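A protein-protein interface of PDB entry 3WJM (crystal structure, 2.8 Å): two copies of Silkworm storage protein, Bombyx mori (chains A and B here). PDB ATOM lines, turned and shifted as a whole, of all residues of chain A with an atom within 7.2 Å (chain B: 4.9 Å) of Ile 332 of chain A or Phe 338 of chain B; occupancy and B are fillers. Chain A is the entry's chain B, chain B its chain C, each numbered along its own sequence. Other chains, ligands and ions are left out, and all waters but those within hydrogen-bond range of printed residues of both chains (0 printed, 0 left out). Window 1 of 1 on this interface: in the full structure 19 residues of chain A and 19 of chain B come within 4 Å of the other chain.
Of the 19 printed residues of chain A, 9 touch a printed residue of chain B.
Hydrophobic or aromatic side chains of chain A that line the printed part of chain B: Ile 332, Tyr 333 and Tyr 367.
Hydrophobic or aromatic side chains of chain B that line the printed part of chain A: Phe 338 and Tyr 434.
NH1 of Arg 328 of chain A lies close to OH of Tyr 434 of chain B, 3.4 Å away.
OD2 of Asp 331 of chain A lies within salt-bridge range of NZ of Lys 335 of chain B (2.6 Å).
OG1 of Thr 336 of chain A lies within hydrogen-bond range of NE2 of Gln 339 of chain B, at 2.8 Å.
The side-chain amide nitrogen (NE2) of Gln 339 of chain B is in hydrogen-bond range of the side-chain amide oxygen (OE1) of Gln 339 of chain A (3.0 Å).
OH of Tyr 367 of chain A is in hydrogen-bond range of NE2 of Gln 342 of chain B (3.3 Å).
The guanidinium group of Arg 385 of chain A lies within salt-bridge range of the side-chain carboxylate of Glu 437 of chain B, 3.3 Å away.
The side-chain carboxylate of Glu 325 of chain A sits close to the side-chain carboxylate of Glu 437 of chain B, 3.3 Å away.
Among the printed residues, pairs that only touch across the chains: Ile 332 of chain A with Phe 338 of chain B (3.1 Å), Ile 332 of chain A with Lys 335 of chain B (3.1 Å), Tyr 333 of chain A with Gln 342 of chain B (3.6 Å), Glu 325 of chain A with Phe 338 of chain B (3.7 Å), Thr 336 of chain A with Gln 342 of chain B (3.7 Å), Ile 332 of chain A with Gln 339 of chain B (3.8 Å) and Arg 328 of chain A with Glu 334 of chain B (3.8 Å).
The side-chain carboxylate of Glu 325 of chain A is in salt-bridge range of the guanidinium group of Arg 385 of chain A, at 2.9 Å.
OD2 of Asp 331 of chain A is in salt-bridge range of NZ of Lys 335 of chain A.
The backbone carbonyl oxygen of Ile 332 of chain A is in hydrogen-bond range of the side-chain hydroxyl of Thr 336 of chain A, 2.8 Å away.
OH of Tyr 333 of chain A sits at hydrogen-bond distance from O of Tyr 367 of chain A (2.6 Å).
OE2 of Glu 334 of chain B sits at hydrogen-bond distance from OH of Tyr 434 of chain B (3.1 Å).
Of chain B, only Lys 335 (3.1 Å), Phe 338 (3.1 Å) and Gln 339 (3.8 Å) come within 4 Å of Ile 332 of chain A.
Phe 338 of chain B touches two residues of chain A.
Of the printed residues of chain A, Tyr 434 of chain B touches Arg 328.
Printed residues of chain B within 4 Å of Arg 385 of chain A: Glu 437.
Of the printed residues of chain A, Gln 342 of chain B touches Tyr 333, Thr 336 and Tyr 367.
Printed residues of chain B within 4 Å of Glu 325 of chain A: Phe 338 (3.7 Å) and Glu 437 (3.3 Å).
Phe 338 of chain A touches none of the printed residues of chain B.
The nearest printed residue of chain B that does not touch Ile 332 of chain A is Thr 336 of chain B (5.4 Å).
The nearest printed residue of chain A that does not touch Gln 339 of chain B is Lys 335 of chain A (5.0 Å).
Thr 336 of chain A touches Gln 339 of chain B, but with the chains exchanged Gln 339 of chain A does not touch Thr 336 of chain B (7.3 Å).
Gln 339 of chain A touches its own counterpart, Gln 339 of chain B.
Positions printed for both chains: 334, 335, 336, 337, 338 and 339.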
ATOM      1  N   TYR A 291      -6.110   7.966  27.410  1.00  0.00           N
ATOM      2  CA  TYR A 291      -4.870   8.214  28.122  1.00  0.00           C
ATOM      3  C   TYR A 291      -4.361   6.968  28.802  1.00  0.00           C
ATOM      4  O   TYR A 291      -3.535   7.068  29.676  1.00  0.00           O
ATOM      5  CB  TYR A 291      -5.039   9.359  29.120  1.00  0.00           C
ATOM      6  CG  TYR A 291      -5.397  10.676  28.441  1.00  0.00           C
ATOM      7  CD1 TYR A 291      -6.745  11.040  28.272  1.00  0.00           C
ATOM      8  CD2 TYR A 291      -4.387  11.569  27.976  1.00  0.00           C
ATOM      9  CE1 TYR A 291      -7.096  12.228  27.651  1.00  0.00           C
ATOM     10  CE2 TYR A 291      -4.725  12.770  27.380  1.00  0.00           C
ATOM     11  CZ  TYR A 291      -6.092  13.084  27.203  1.00  0.00           C
ATOM     12  OH  TYR A 291      -6.498  14.268  26.622  1.00  0.00           O
ATOM     13  N   GLU A 325      -1.361  14.795  19.490  1.00  0.00           N
ATOM     14  CA  GLU A 325      -2.151  15.811  18.840  1.00  0.00           C
ATOM     15  C   GLU A 325      -3.555  15.312  18.577  1.00  0.00           C
ATOM     16  O   GLU A 325      -4.529  16.041  18.831  1.00  0.00           O
ATOM     17  CB  GLU A 325      -1.477  16.340  17.564  1.00  0.00           C
ATOM     18  CG  GLU A 325      -2.159  17.564  16.947  1.00  0.00           C
ATOM     19  CD  GLU A 325      -3.459  17.223  16.208  1.00  0.00           C
ATOM     20  OE1 GLU A 325      -3.473  16.238  15.434  1.00  0.00           O
ATOM     21  OE2 GLU A 325      -4.495  17.919  16.402  1.00  0.00           O
ATOM     22  N   GLU A 326      -3.663  14.077  18.090  1.00  0.00           N
ATOM     23  CA  GLU A 326      -4.969  13.478  17.733  1.00  0.00           C
ATOM     24  C   GLU A 326      -5.843  13.248  18.971  1.00  0.00           C
ATOM     25  O   GLU A 326      -7.063  13.484  18.928  1.00  0.00           O
ATOM     26  CB  GLU A 326      -4.773  12.181  16.960  1.00  0.00           C
ATOM     27  CG  GLU A 326      -4.583  12.393  15.475  1.00  0.00           C
ATOM     28  CD  GLU A 326      -3.414  11.623  14.883  1.00  0.00           C
ATOM     29  OE1 GLU A 326      -3.251  10.417  15.135  1.00  0.00           O
ATOM     30  OE2 GLU A 326      -2.650  12.237  14.124  1.00  0.00           O
ATOM     31  N   ILE A 327      -5.212  12.823  20.077  1.00  0.00           N
ATOM     32  CA  ILE A 327      -5.914  12.626  21.351  1.00  0.00           C
ATOM     33  C   ILE A 327      -6.476  13.921  21.884  1.00  0.00           C
ATOM     34  O   ILE A 327      -7.586  13.939  22.426  1.00  0.00           O
ATOM     35  CB  ILE A 327      -5.025  11.952  22.413  1.00  0.00           C
ATOM     36  CG1 ILE A 327      -4.989  10.459  22.145  1.00  0.00           C
ATOM     37  CG2 ILE A 327      -5.559  12.175  23.827  1.00  0.00           C
ATOM     38  CD1 ILE A 327      -3.658   9.870  22.494  1.00  0.00           C
ATOM     39  N   ARG A 328      -5.710  14.998  21.715  1.00  0.00           N
ATOM     40  CA  ARG A 328      -6.192  16.319  22.083  1.00  0.00           C
ATOM     41  C   ARG A 328      -7.496  16.607  21.376  1.00  0.00           C
ATOM     42  O   ARG A 328      -8.490  16.929  22.031  1.00  0.00           O
ATOM     43  CB  ARG A 328      -5.155  17.382  21.806  1.00  0.00           C
ATOM     44  CG  ARG A 328      -4.377  17.732  23.038  1.00  0.00           C
ATOM     45  CD  ARG A 328      -3.413  18.835  22.750  1.00  0.00           C
ATOM     46  NE  ARG A 328      -2.046  18.349  22.681  1.00  0.00           N
ATOM     47  CZ  ARG A 328      -1.231  18.450  21.624  1.00  0.00           C
ATOM     48  NH1 ARG A 328      -1.614  19.028  20.490  1.00  0.00           N
ATOM     49  NH2 ARG A 328       0.006  17.963  21.727  1.00  0.00           N
ATOM     50  N   PHE A 329      -7.492  16.414  20.059  1.00  0.00           N
ATOM     51  CA  PHE A 329      -8.684  16.546  19.226  1.00  0.00           C
ATOM     52  C   PHE A 329      -9.862  15.669  19.677  1.00  0.00           C
ATOM     53  O   PHE A 329     -10.971  16.156  19.874  1.00  0.00           O
ATOM     54  CB  PHE A 329      -8.368  16.270  17.755  1.00  0.00           C
ATOM     55  CG  PHE A 329      -9.585  16.235  16.895  1.00  0.00           C
ATOM     56  CD1 PHE A 329     -10.268  17.415  16.574  1.00  0.00           C
ATOM     57  CD2 PHE A 329     -10.100  15.022  16.439  1.00  0.00           C
ATOM     58  CE1 PHE A 329     -11.418  17.385  15.790  1.00  0.00           C
ATOM     59  CE2 PHE A 329     -11.259  14.990  15.643  1.00  0.00           C
ATOM     60  CZ  PHE A 329     -11.924  16.175  15.329  1.00  0.00           C
ATOM     61  N   LEU A 330      -9.619  14.378  19.835  1.00  0.00           N
ATOM     62  CA  LEU A 330     -10.669  13.468  20.249  1.00  0.00           C
ATOM     63  C   LEU A 330     -11.193  13.824  21.628  1.00  0.00           C
ATOM     64  O   LEU A 330     -12.379  13.680  21.921  1.00  0.00           O
ATOM     65  CB  LEU A 330     -10.157  12.033  20.221  1.00  0.00           C
ATOM     66  CG  LEU A 330      -9.726  11.450  18.862  1.00  0.00           C
ATOM     67  CD1 LEU A 330      -8.841  10.244  19.160  1.00  0.00           C
ATOM     68  CD2 LEU A 330     -10.895  11.059  17.961  1.00  0.00           C
ATOM     69  N   ASP A 331     -10.309  14.329  22.473  1.00  0.00           N
ATOM     70  CA  ASP A 331     -10.695  14.639  23.836  1.00  0.00           C
ATOM     71  C   ASP A 331     -11.677  15.817  23.897  1.00  0.00           C
ATOM     72  O   ASP A 331     -12.624  15.776  24.711  1.00  0.00           O
ATOM     73  CB  ASP A 331      -9.460  14.890  24.699  1.00  0.00           C
ATOM     74  CG  ASP A 331      -9.792  15.040  26.164  1.00  0.00           C
ATOM     75  OD1 ASP A 331     -10.334  14.094  26.791  1.00  0.00           O
ATOM     76  OD2 ASP A 331      -9.521  16.123  26.715  1.00  0.00           O
ATOM     77  N   ILE A 332     -11.486  16.849  23.065  1.00  0.00           N
ATOM     78  CA  ILE A 332     -12.402  17.979  23.158  1.00  0.00           C
ATOM     79  C   ILE A 332     -13.670  17.678  22.430  1.00  0.00           C
ATOM     80  O   ILE A 332     -14.740  18.165  22.816  1.00  0.00           O
ATOM     81  CB  ILE A 332     -11.916  19.254  22.497  1.00  0.00           C
ATOM     82  CG1 ILE A 332     -10.436  19.186  22.273  1.00  0.00           C
ATOM     83  CG2 ILE A 332     -12.450  20.479  23.208  1.00  0.00           C
ATOM     84  CD1 ILE A 332     -10.214  19.048  20.786  1.00  0.00           C
ATOM     85  N   TYR A 333     -13.544  16.906  21.362  1.00  0.00           N
ATOM     86  CA  TYR A 333     -14.699  16.515  20.607  1.00  0.00           C
ATOM     87  C   TYR A 333     -15.693  15.824  21.549  1.00  0.00           C
ATOM     88  O   TYR A 333     -16.894  16.140  21.522  1.00  0.00           O
ATOM     89  CB  TYR A 333     -14.293  15.588  19.487  1.00  0.00           C
ATOM     90  CG  TYR A 333     -15.237  15.615  18.330  1.00  0.00           C
ATOM     91  CD1 TYR A 333     -14.898  16.243  17.147  1.00  0.00           C
ATOM     92  CD2 TYR A 333     -16.481  15.002  18.419  1.00  0.00           C
ATOM     93  CE1 TYR A 333     -15.779  16.248  16.078  1.00  0.00           C
ATOM     94  CE2 TYR A 333     -17.385  15.027  17.370  1.00  0.00           C
ATOM     95  CZ  TYR A 333     -17.030  15.636  16.191  1.00  0.00           C
ATOM     96  OH  TYR A 333     -17.944  15.631  15.151  1.00  0.00           O
ATOM     97  N   GLU A 334     -15.188  14.932  22.412  1.00  0.00           N
ATOM     98  CA  GLU A 334     -15.996  14.308  23.463  1.00  0.00           C
ATOM     99  C   GLU A 334     -16.500  15.301  24.500  1.00  0.00           C
ATOM    100  O   GLU A 334     -17.698  15.330  24.844  1.00  0.00           O
ATOM    101  CB  GLU A 334     -15.214  13.175  24.136  1.00  0.00           C
ATOM    102  CG  GLU A 334     -14.795  12.112  23.132  1.00  0.00           C
ATOM    103  CD  GLU A 334     -14.228  10.845  23.743  1.00  0.00           C
ATOM    104  OE1 GLU A 334     -14.029   9.882  22.975  1.00  0.00           O
ATOM    105  OE2 GLU A 334     -13.966  10.797  24.966  1.00  0.00           O
ATOM    106  N   LYS A 335     -15.599  16.139  24.998  1.00  0.00           N
ATOM    107  CA  LYS A 335     -15.982  17.031  26.079  1.00  0.00           C
ATOM    108  C   LYS A 335     -16.961  18.120  25.667  1.00  0.00           C
ATOM    109  O   LYS A 335     -17.787  18.537  26.468  1.00  0.00           O
ATOM    110  CB  LYS A 335     -14.759  17.579  26.786  1.00  0.00           C
ATOM    111  CG  LYS A 335     -14.261  16.558  27.780  1.00  0.00           C
ATOM    112  CD  LYS A 335     -12.826  16.798  28.224  1.00  0.00           C
ATOM    113  CE  LYS A 335     -12.260  15.453  28.655  1.00  0.00           C
ATOM    114  NZ  LYS A 335     -10.944  15.620  29.321  1.00  0.00           N
ATOM    115  N   THR A 336     -16.874  18.556  24.414  1.00  0.00           N
ATOM    116  CA  THR A 336     -17.871  19.441  23.823  1.00  0.00           C
ATOM    117  C   THR A 336     -19.265  18.842  23.953  1.00  0.00           C
ATOM    118  O   THR A 336     -20.206  19.544  24.380  1.00  0.00           O
ATOM    119  CB  THR A 336     -17.523  19.732  22.355  1.00  0.00           C
ATOM    120  OG1 THR A 336     -16.275  20.438  22.329  1.00  0.00           O
ATOM    121  CG2 THR A 336     -18.622  20.577  21.635  1.00  0.00           C
ATOM    122  N   PHE A 337     -19.380  17.551  23.610  1.00  0.00           N
ATOM    123  CA  PHE A 337     -20.596  16.787  23.859  1.00  0.00           C
ATOM    124  C   PHE A 337     -21.108  16.813  25.329  1.00  0.00           C
ATOM    125  O   PHE A 337     -22.298  17.151  25.575  1.00  0.00           O
ATOM    126  CB  PHE A 337     -20.520  15.367  23.299  1.00  0.00           C
ATOM    127  CG  PHE A 337     -21.871  14.699  23.196  1.00  0.00           C
ATOM    128  CD1 PHE A 337     -22.775  15.060  22.191  1.00  0.00           C
ATOM    129  CD2 PHE A 337     -22.265  13.739  24.113  1.00  0.00           C
ATOM    130  CE1 PHE A 337     -24.029  14.468  22.101  1.00  0.00           C
ATOM    131  CE2 PHE A 337     -23.526  13.142  24.034  1.00  0.00           C
ATOM    132  CZ  PHE A 337     -24.412  13.512  23.025  1.00  0.00           C
ATOM    133  N   PHE A 338     -20.224  16.521  26.289  1.00  0.00           N
ATOM    134  CA  PHE A 338     -20.575  16.649  27.719  1.00  0.00           C
ATOM    135  C   PHE A 338     -21.150  18.020  28.038  1.00  0.00           C
ATOM    136  O   PHE A 338     -22.193  18.139  28.672  1.00  0.00           O
ATOM    137  CB  PHE A 338     -19.370  16.416  28.624  1.00  0.00           C
ATOM    138  CG  PHE A 338     -19.109  14.974  28.949  1.00  0.00           C
ATOM    139  CD1 PHE A 338     -18.086  14.274  28.314  1.00  0.00           C
ATOM    140  CD2 PHE A 338     -19.865  14.311  29.927  1.00  0.00           C
ATOM    141  CE1 PHE A 338     -17.820  12.932  28.629  1.00  0.00           C
ATOM    142  CE2 PHE A 338     -19.606  12.962  30.256  1.00  0.00           C
ATOM    143  CZ  PHE A 338     -18.585  12.266  29.607  1.00  0.00           C
ATOM    144  N   GLN A 339     -20.477  19.061  27.580  1.00  0.00           N
ATOM    145  CA  GLN A 339     -20.939  20.418  27.777  1.00  0.00           C
ATOM    146  C   GLN A 339     -22.342  20.639  27.200  1.00  0.00           C
ATOM    147  O   GLN A 339     -23.149  21.361  27.815  1.00  0.00           O
ATOM    148  CB  GLN A 339     -19.947  21.436  27.184  1.00  0.00           C
ATOM    149  CG  GLN A 339     -18.581  21.474  27.839  1.00  0.00           C
ATOM    150  CD  GLN A 339     -17.773  22.693  27.406  1.00  0.00           C
ATOM    151  OE1 GLN A 339     -17.567  22.903  26.217  1.00  0.00           O
ATOM    152  NE2 GLN A 339     -17.311  23.502  28.375  1.00  0.00           N
ATOM    153  N   TYR A 367     -23.699  14.825  14.745  1.00  0.00           N
ATOM    154  CA  TYR A 367     -22.556  15.332  15.496  1.00  0.00           C
ATOM    155  C   TYR A 367     -21.483  14.287  15.588  1.00  0.00           C
ATOM    156  O   TYR A 367     -20.299  14.556  15.403  1.00  0.00           O
ATOM    157  CB  TYR A 367     -22.954  15.654  16.928  1.00  0.00           C
ATOM    158  CG  TYR A 367     -21.755  16.111  17.704  1.00  0.00           C
ATOM    159  CD1 TYR A 367     -21.214  17.372  17.474  1.00  0.00           C
ATOM    160  CD2 TYR A 367     -21.110  15.262  18.618  1.00  0.00           C
ATOM    161  CE1 TYR A 367     -20.092  17.785  18.155  1.00  0.00           C
ATOM    162  CE2 TYR A 367     -19.970  15.673  19.283  1.00  0.00           C
ATOM    163  CZ  TYR A 367     -19.460  16.928  19.042  1.00  0.00           C
ATOM    164  OH  TYR A 367     -18.338  17.395  19.705  1.00  0.00           O
ATOM    165  N   ARG A 385     -12.711  18.193  10.536  1.00  0.00           N
ATOM    166  CA  ARG A 385     -12.069  16.966  11.018  1.00  0.00           C
ATOM    167  C   ARG A 385     -13.067  16.033  11.650  1.00  0.00           C
ATOM    168  O   ARG A 385     -13.973  16.468  12.369  1.00  0.00           O
ATOM    169  CB  ARG A 385     -11.008  17.281  12.061  1.00  0.00           C
ATOM    170  CG  ARG A 385      -9.761  17.940  11.524  1.00  0.00           C
ATOM    171  CD  ARG A 385      -8.820  18.315  12.666  1.00  0.00           C
ATOM    172  NE  ARG A 385      -8.004  17.168  13.076  1.00  0.00           N
ATOM    173  CZ  ARG A 385      -7.058  17.208  14.023  1.00  0.00           C
ATOM    174  NH1 ARG A 385      -6.794  18.342  14.675  1.00  0.00           N
ATOM    175  NH2 ARG A 385      -6.373  16.106  14.313  1.00  0.00           N
ATOM    176  N   TYR A 387     -14.244  12.913  14.127  1.00  0.00           N
ATOM    177  CA  TYR A 387     -13.958  12.138  15.305  1.00  0.00           C
ATOM    178  C   TYR A 387     -13.694  10.708  14.901  1.00  0.00           C
ATOM    179  O   TYR A 387     -12.663  10.139  15.275  1.00  0.00           O
ATOM    180  CB  TYR A 387     -15.120  12.199  16.283  1.00  0.00           C
ATOM    181  CG  TYR A 387     -14.974  11.316  17.505  1.00  0.00           C
ATOM    182  CD1 TYR A 387     -14.292  11.767  18.626  1.00  0.00           C
ATOM    183  CD2 TYR A 387     -15.534  10.033  17.545  1.00  0.00           C
ATOM    184  CE1 TYR A 387     -14.174  10.968  19.759  1.00  0.00           C
ATOM    185  CE2 TYR A 387     -15.415   9.245  18.658  1.00  0.00           C
ATOM    186  CZ  TYR A 387     -14.738   9.712  19.771  1.00  0.00           C
ATOM    187  OH  TYR A 387     -14.597   8.913  20.907  1.00  0.00           O
ATOM    188  N   GLU B 334      -6.131  25.686  25.212  1.00  0.00           N
ATOM    189  CA  GLU B 334      -5.966  25.129  23.890  1.00  0.00           C
ATOM    190  C   GLU B 334      -7.307  24.602  23.358  1.00  0.00           C
ATOM    191  O   GLU B 334      -7.745  24.936  22.263  1.00  0.00           O
ATOM    192  CB  GLU B 334      -4.916  24.010  23.945  1.00  0.00           C
ATOM    193  CG  GLU B 334      -3.671  24.410  24.735  1.00  0.00           C
ATOM    194  CD  GLU B 334      -2.515  23.415  24.682  1.00  0.00           C
ATOM    195  OE1 GLU B 334      -1.352  23.840  24.857  1.00  0.00           O
ATOM    196  OE2 GLU B 334      -2.765  22.212  24.480  1.00  0.00           O
ATOM    197  N   LYS B 335      -7.981  23.779  24.137  1.00  0.00           N
ATOM    198  CA  LYS B 335      -9.217  23.184  23.652  1.00  0.00           C
ATOM    199  C   LYS B 335     -10.305  24.207  23.332  1.00  0.00           C
ATOM    200  O   LYS B 335     -11.105  23.954  22.452  1.00  0.00           O
ATOM    201  CB  LYS B 335      -9.708  22.079  24.590  1.00  0.00           C
ATOM    202  CG  LYS B 335      -8.874  20.816  24.441  1.00  0.00           C
ATOM    203  CD  LYS B 335      -9.130  19.750  25.499  1.00  0.00           C
ATOM    204  CE  LYS B 335      -7.915  18.821  25.510  1.00  0.00           C
ATOM    205  NZ  LYS B 335      -7.805  18.050  26.773  1.00  0.00           N
ATOM    206  N   THR B 336     -10.301  25.362  24.006  1.00  0.00           N
ATOM    207  CA  THR B 336     -11.213  26.455  23.675  1.00  0.00           C
ATOM    208  C   THR B 336     -10.994  26.898  22.238  1.00  0.00           C
ATOM    209  O   THR B 336     -11.967  27.110  21.497  1.00  0.00           O
ATOM    210  CB  THR B 336     -11.119  27.664  24.648  1.00  0.00           C
ATOM    211  OG1 THR B 336     -11.558  27.270  25.957  1.00  0.00           O
ATOM    212  CG2 THR B 336     -12.015  28.825  24.179  1.00  0.00           C
ATOM    213  N   PHE B 337      -9.734  27.001  21.835  1.00  0.00           N
ATOM    214  CA  PHE B 337      -9.388  27.313  20.458  1.00  0.00           C
ATOM    215  C   PHE B 337      -9.965  26.279  19.497  1.00  0.00           C
ATOM    216  O   PHE B 337     -10.683  26.645  18.541  1.00  0.00           O
ATOM    217  CB  PHE B 337      -7.879  27.368  20.296  1.00  0.00           C
ATOM    218  CG  PHE B 337      -7.420  27.961  18.998  1.00  0.00           C
ATOM    219  CD1 PHE B 337      -7.464  29.334  18.787  1.00  0.00           C
ATOM    220  CD2 PHE B 337      -6.902  27.152  18.004  1.00  0.00           C
ATOM    221  CE1 PHE B 337      -7.021  29.896  17.601  1.00  0.00           C
ATOM    222  CE2 PHE B 337      -6.453  27.699  16.801  1.00  0.00           C
ATOM    223  CZ  PHE B 337      -6.506  29.078  16.600  1.00  0.00           C
ATOM    224  N   PHE B 338      -9.664  25.000  19.756  1.00  0.00           N
ATOM    225  CA  PHE B 338     -10.252  23.904  18.978  1.00  0.00           C
ATOM    226  C   PHE B 338     -11.775  24.033  18.819  1.00  0.00           C
ATOM    227  O   PHE B 338     -12.304  23.776  17.757  1.00  0.00           O
ATOM    228  CB  PHE B 338      -9.887  22.542  19.579  1.00  0.00           C
ATOM    229  CG  PHE B 338      -8.604  21.931  19.028  1.00  0.00           C
ATOM    230  CD1 PHE B 338      -7.938  20.905  19.734  1.00  0.00           C
ATOM    231  CD2 PHE B 338      -8.049  22.356  17.808  1.00  0.00           C
ATOM    232  CE1 PHE B 338      -6.766  20.312  19.231  1.00  0.00           C
ATOM    233  CE2 PHE B 338      -6.877  21.772  17.313  1.00  0.00           C
ATOM    234  CZ  PHE B 338      -6.236  20.745  18.018  1.00  0.00           C
ATOM    235  N   GLN B 339     -12.467  24.463  19.862  1.00  0.00           N
ATOM    236  CA  GLN B 339     -13.928  24.580  19.832  1.00  0.00           C
ATOM    237  C   GLN B 339     -14.440  25.699  18.905  1.00  0.00           C
ATOM    238  O   GLN B 339     -15.453  25.549  18.188  1.00  0.00           O
ATOM    239  CB  GLN B 339     -14.475  24.784  21.236  1.00  0.00           C
ATOM    240  CG  GLN B 339     -14.373  23.547  22.089  1.00  0.00           C
ATOM    241  CD  GLN B 339     -15.056  23.694  23.438  1.00  0.00           C
ATOM    242  OE1 GLN B 339     -14.957  24.729  24.069  1.00  0.00           O
ATOM    243  NE2 GLN B 339     -15.755  22.652  23.882  1.00  0.00           N
ATOM    244  N   TYR B 340     -13.747  26.833  18.939  1.00  0.00           N
ATOM    245  CA  TYR B 340     -13.948  27.885  17.951  1.00  0.00           C
ATOM    246  C   TYR B 340     -13.869  27.304  16.553  1.00  0.00           C
ATOM    247  O   TYR B 340     -14.802  27.387  15.771  1.00  0.00           O
ATOM    248  CB  TYR B 340     -12.859  28.932  18.109  1.00  0.00           C
ATOM    249  CG  TYR B 340     -12.911  29.700  19.395  1.00  0.00           C
ATOM    250  CD1 TYR B 340     -11.736  30.188  19.974  1.00  0.00           C
ATOM    251  CD2 TYR B 340     -14.132  29.946  20.034  1.00  0.00           C
ATOM    252  CE1 TYR B 340     -11.777  30.917  21.153  1.00  0.00           C
ATOM    253  CE2 TYR B 340     -14.197  30.659  21.210  1.00  0.00           C
ATOM    254  CZ  TYR B 340     -13.015  31.140  21.777  1.00  0.00           C
ATOM    255  OH  TYR B 340     -13.073  31.872  22.959  1.00  0.00           O
ATOM    256  N   LEU B 341     -12.733  26.704  16.243  1.00  0.00           N
ATOM    257  CA  LEU B 341     -12.541  26.117  14.930  1.00  0.00           C
ATOM    258  C   LEU B 341     -13.627  25.131  14.594  1.00  0.00           C
ATOM    259  O   LEU B 341     -14.144  25.158  13.488  1.00  0.00           O
ATOM    260  CB  LEU B 341     -11.178  25.441  14.817  1.00  0.00           C
ATOM    261  CG  LEU B 341     -10.039  26.411  15.050  1.00  0.00           C
ATOM    262  CD1 LEU B 341      -8.736  25.738  14.624  1.00  0.00           C
ATOM    263  CD2 LEU B 341     -10.334  27.733  14.312  1.00  0.00           C
ATOM    264  N   GLN B 342     -13.987  24.274  15.545  1.00  0.00           N
ATOM    265  CA  GLN B 342     -15.036  23.299  15.290  1.00  0.00           C
ATOM    266  C   GLN B 342     -16.312  24.021  14.900  1.00  0.00           C
ATOM    267  O   GLN B 342     -17.042  23.556  14.046  1.00  0.00           O
ATOM    268  CB  GLN B 342     -15.267  22.390  16.491  1.00  0.00           C
ATOM    269  CG  GLN B 342     -16.285  21.289  16.220  1.00  0.00           C
ATOM    270  CD  GLN B 342     -16.710  20.593  17.495  1.00  0.00           C
ATOM    271  OE1 GLN B 342     -16.634  21.173  18.577  1.00  0.00           O
ATOM    272  NE2 GLN B 342     -17.150  19.350  17.381  1.00  0.00           N
ATOM    273  N   TYR B 434      -0.982  25.127  16.194  1.00  0.00           N
ATOM    274  CA  TYR B 434      -2.369  25.507  16.386  1.00  0.00           C
ATOM    275  C   TYR B 434      -2.829  26.610  15.442  1.00  0.00           C
ATOM    276  O   TYR B 434      -3.921  26.527  14.877  1.00  0.00           O
ATOM    277  CB  TYR B 434      -2.589  25.964  17.807  1.00  0.00           C
ATOM    278  CG  TYR B 434      -2.801  24.840  18.764  1.00  0.00           C
ATOM    279  CD1 TYR B 434      -2.059  24.752  19.919  1.00  0.00           C
ATOM    280  CD2 TYR B 434      -3.749  23.860  18.515  1.00  0.00           C
ATOM    281  CE1 TYR B 434      -2.245  23.734  20.813  1.00  0.00           C
ATOM    282  CE2 TYR B 434      -3.932  22.826  19.404  1.00  0.00           C
ATOM    283  CZ  TYR B 434      -3.169  22.773  20.551  1.00  0.00           C
ATOM    284  OH  TYR B 434      -3.365  21.766  21.473  1.00  0.00           O
ATOM    285  N   GLU B 437      -3.416  25.263  12.121  1.00  0.00           N
ATOM    286  CA  GLU B 437      -4.663  24.543  11.986  1.00  0.00           C
ATOM    287  C   GLU B 437      -5.770  25.511  11.578  1.00  0.00           C
ATOM    288  O   GLU B 437      -6.595  25.166  10.744  1.00  0.00           O
ATOM    289  CB  GLU B 437      -5.016  23.758  13.247  1.00  0.00           C
ATOM    290  CG  GLU B 437      -4.058  22.610  13.535  1.00  0.00           C
ATOM    291  CD  GLU B 437      -4.609  21.598  14.538  1.00  0.00           C
ATOM    292  OE1 GLU B 437      -5.848  21.465  14.590  1.00  0.00           O
ATOM    293  OE2 GLU B 437      -3.820  20.926  15.261  1.00  0.00           O
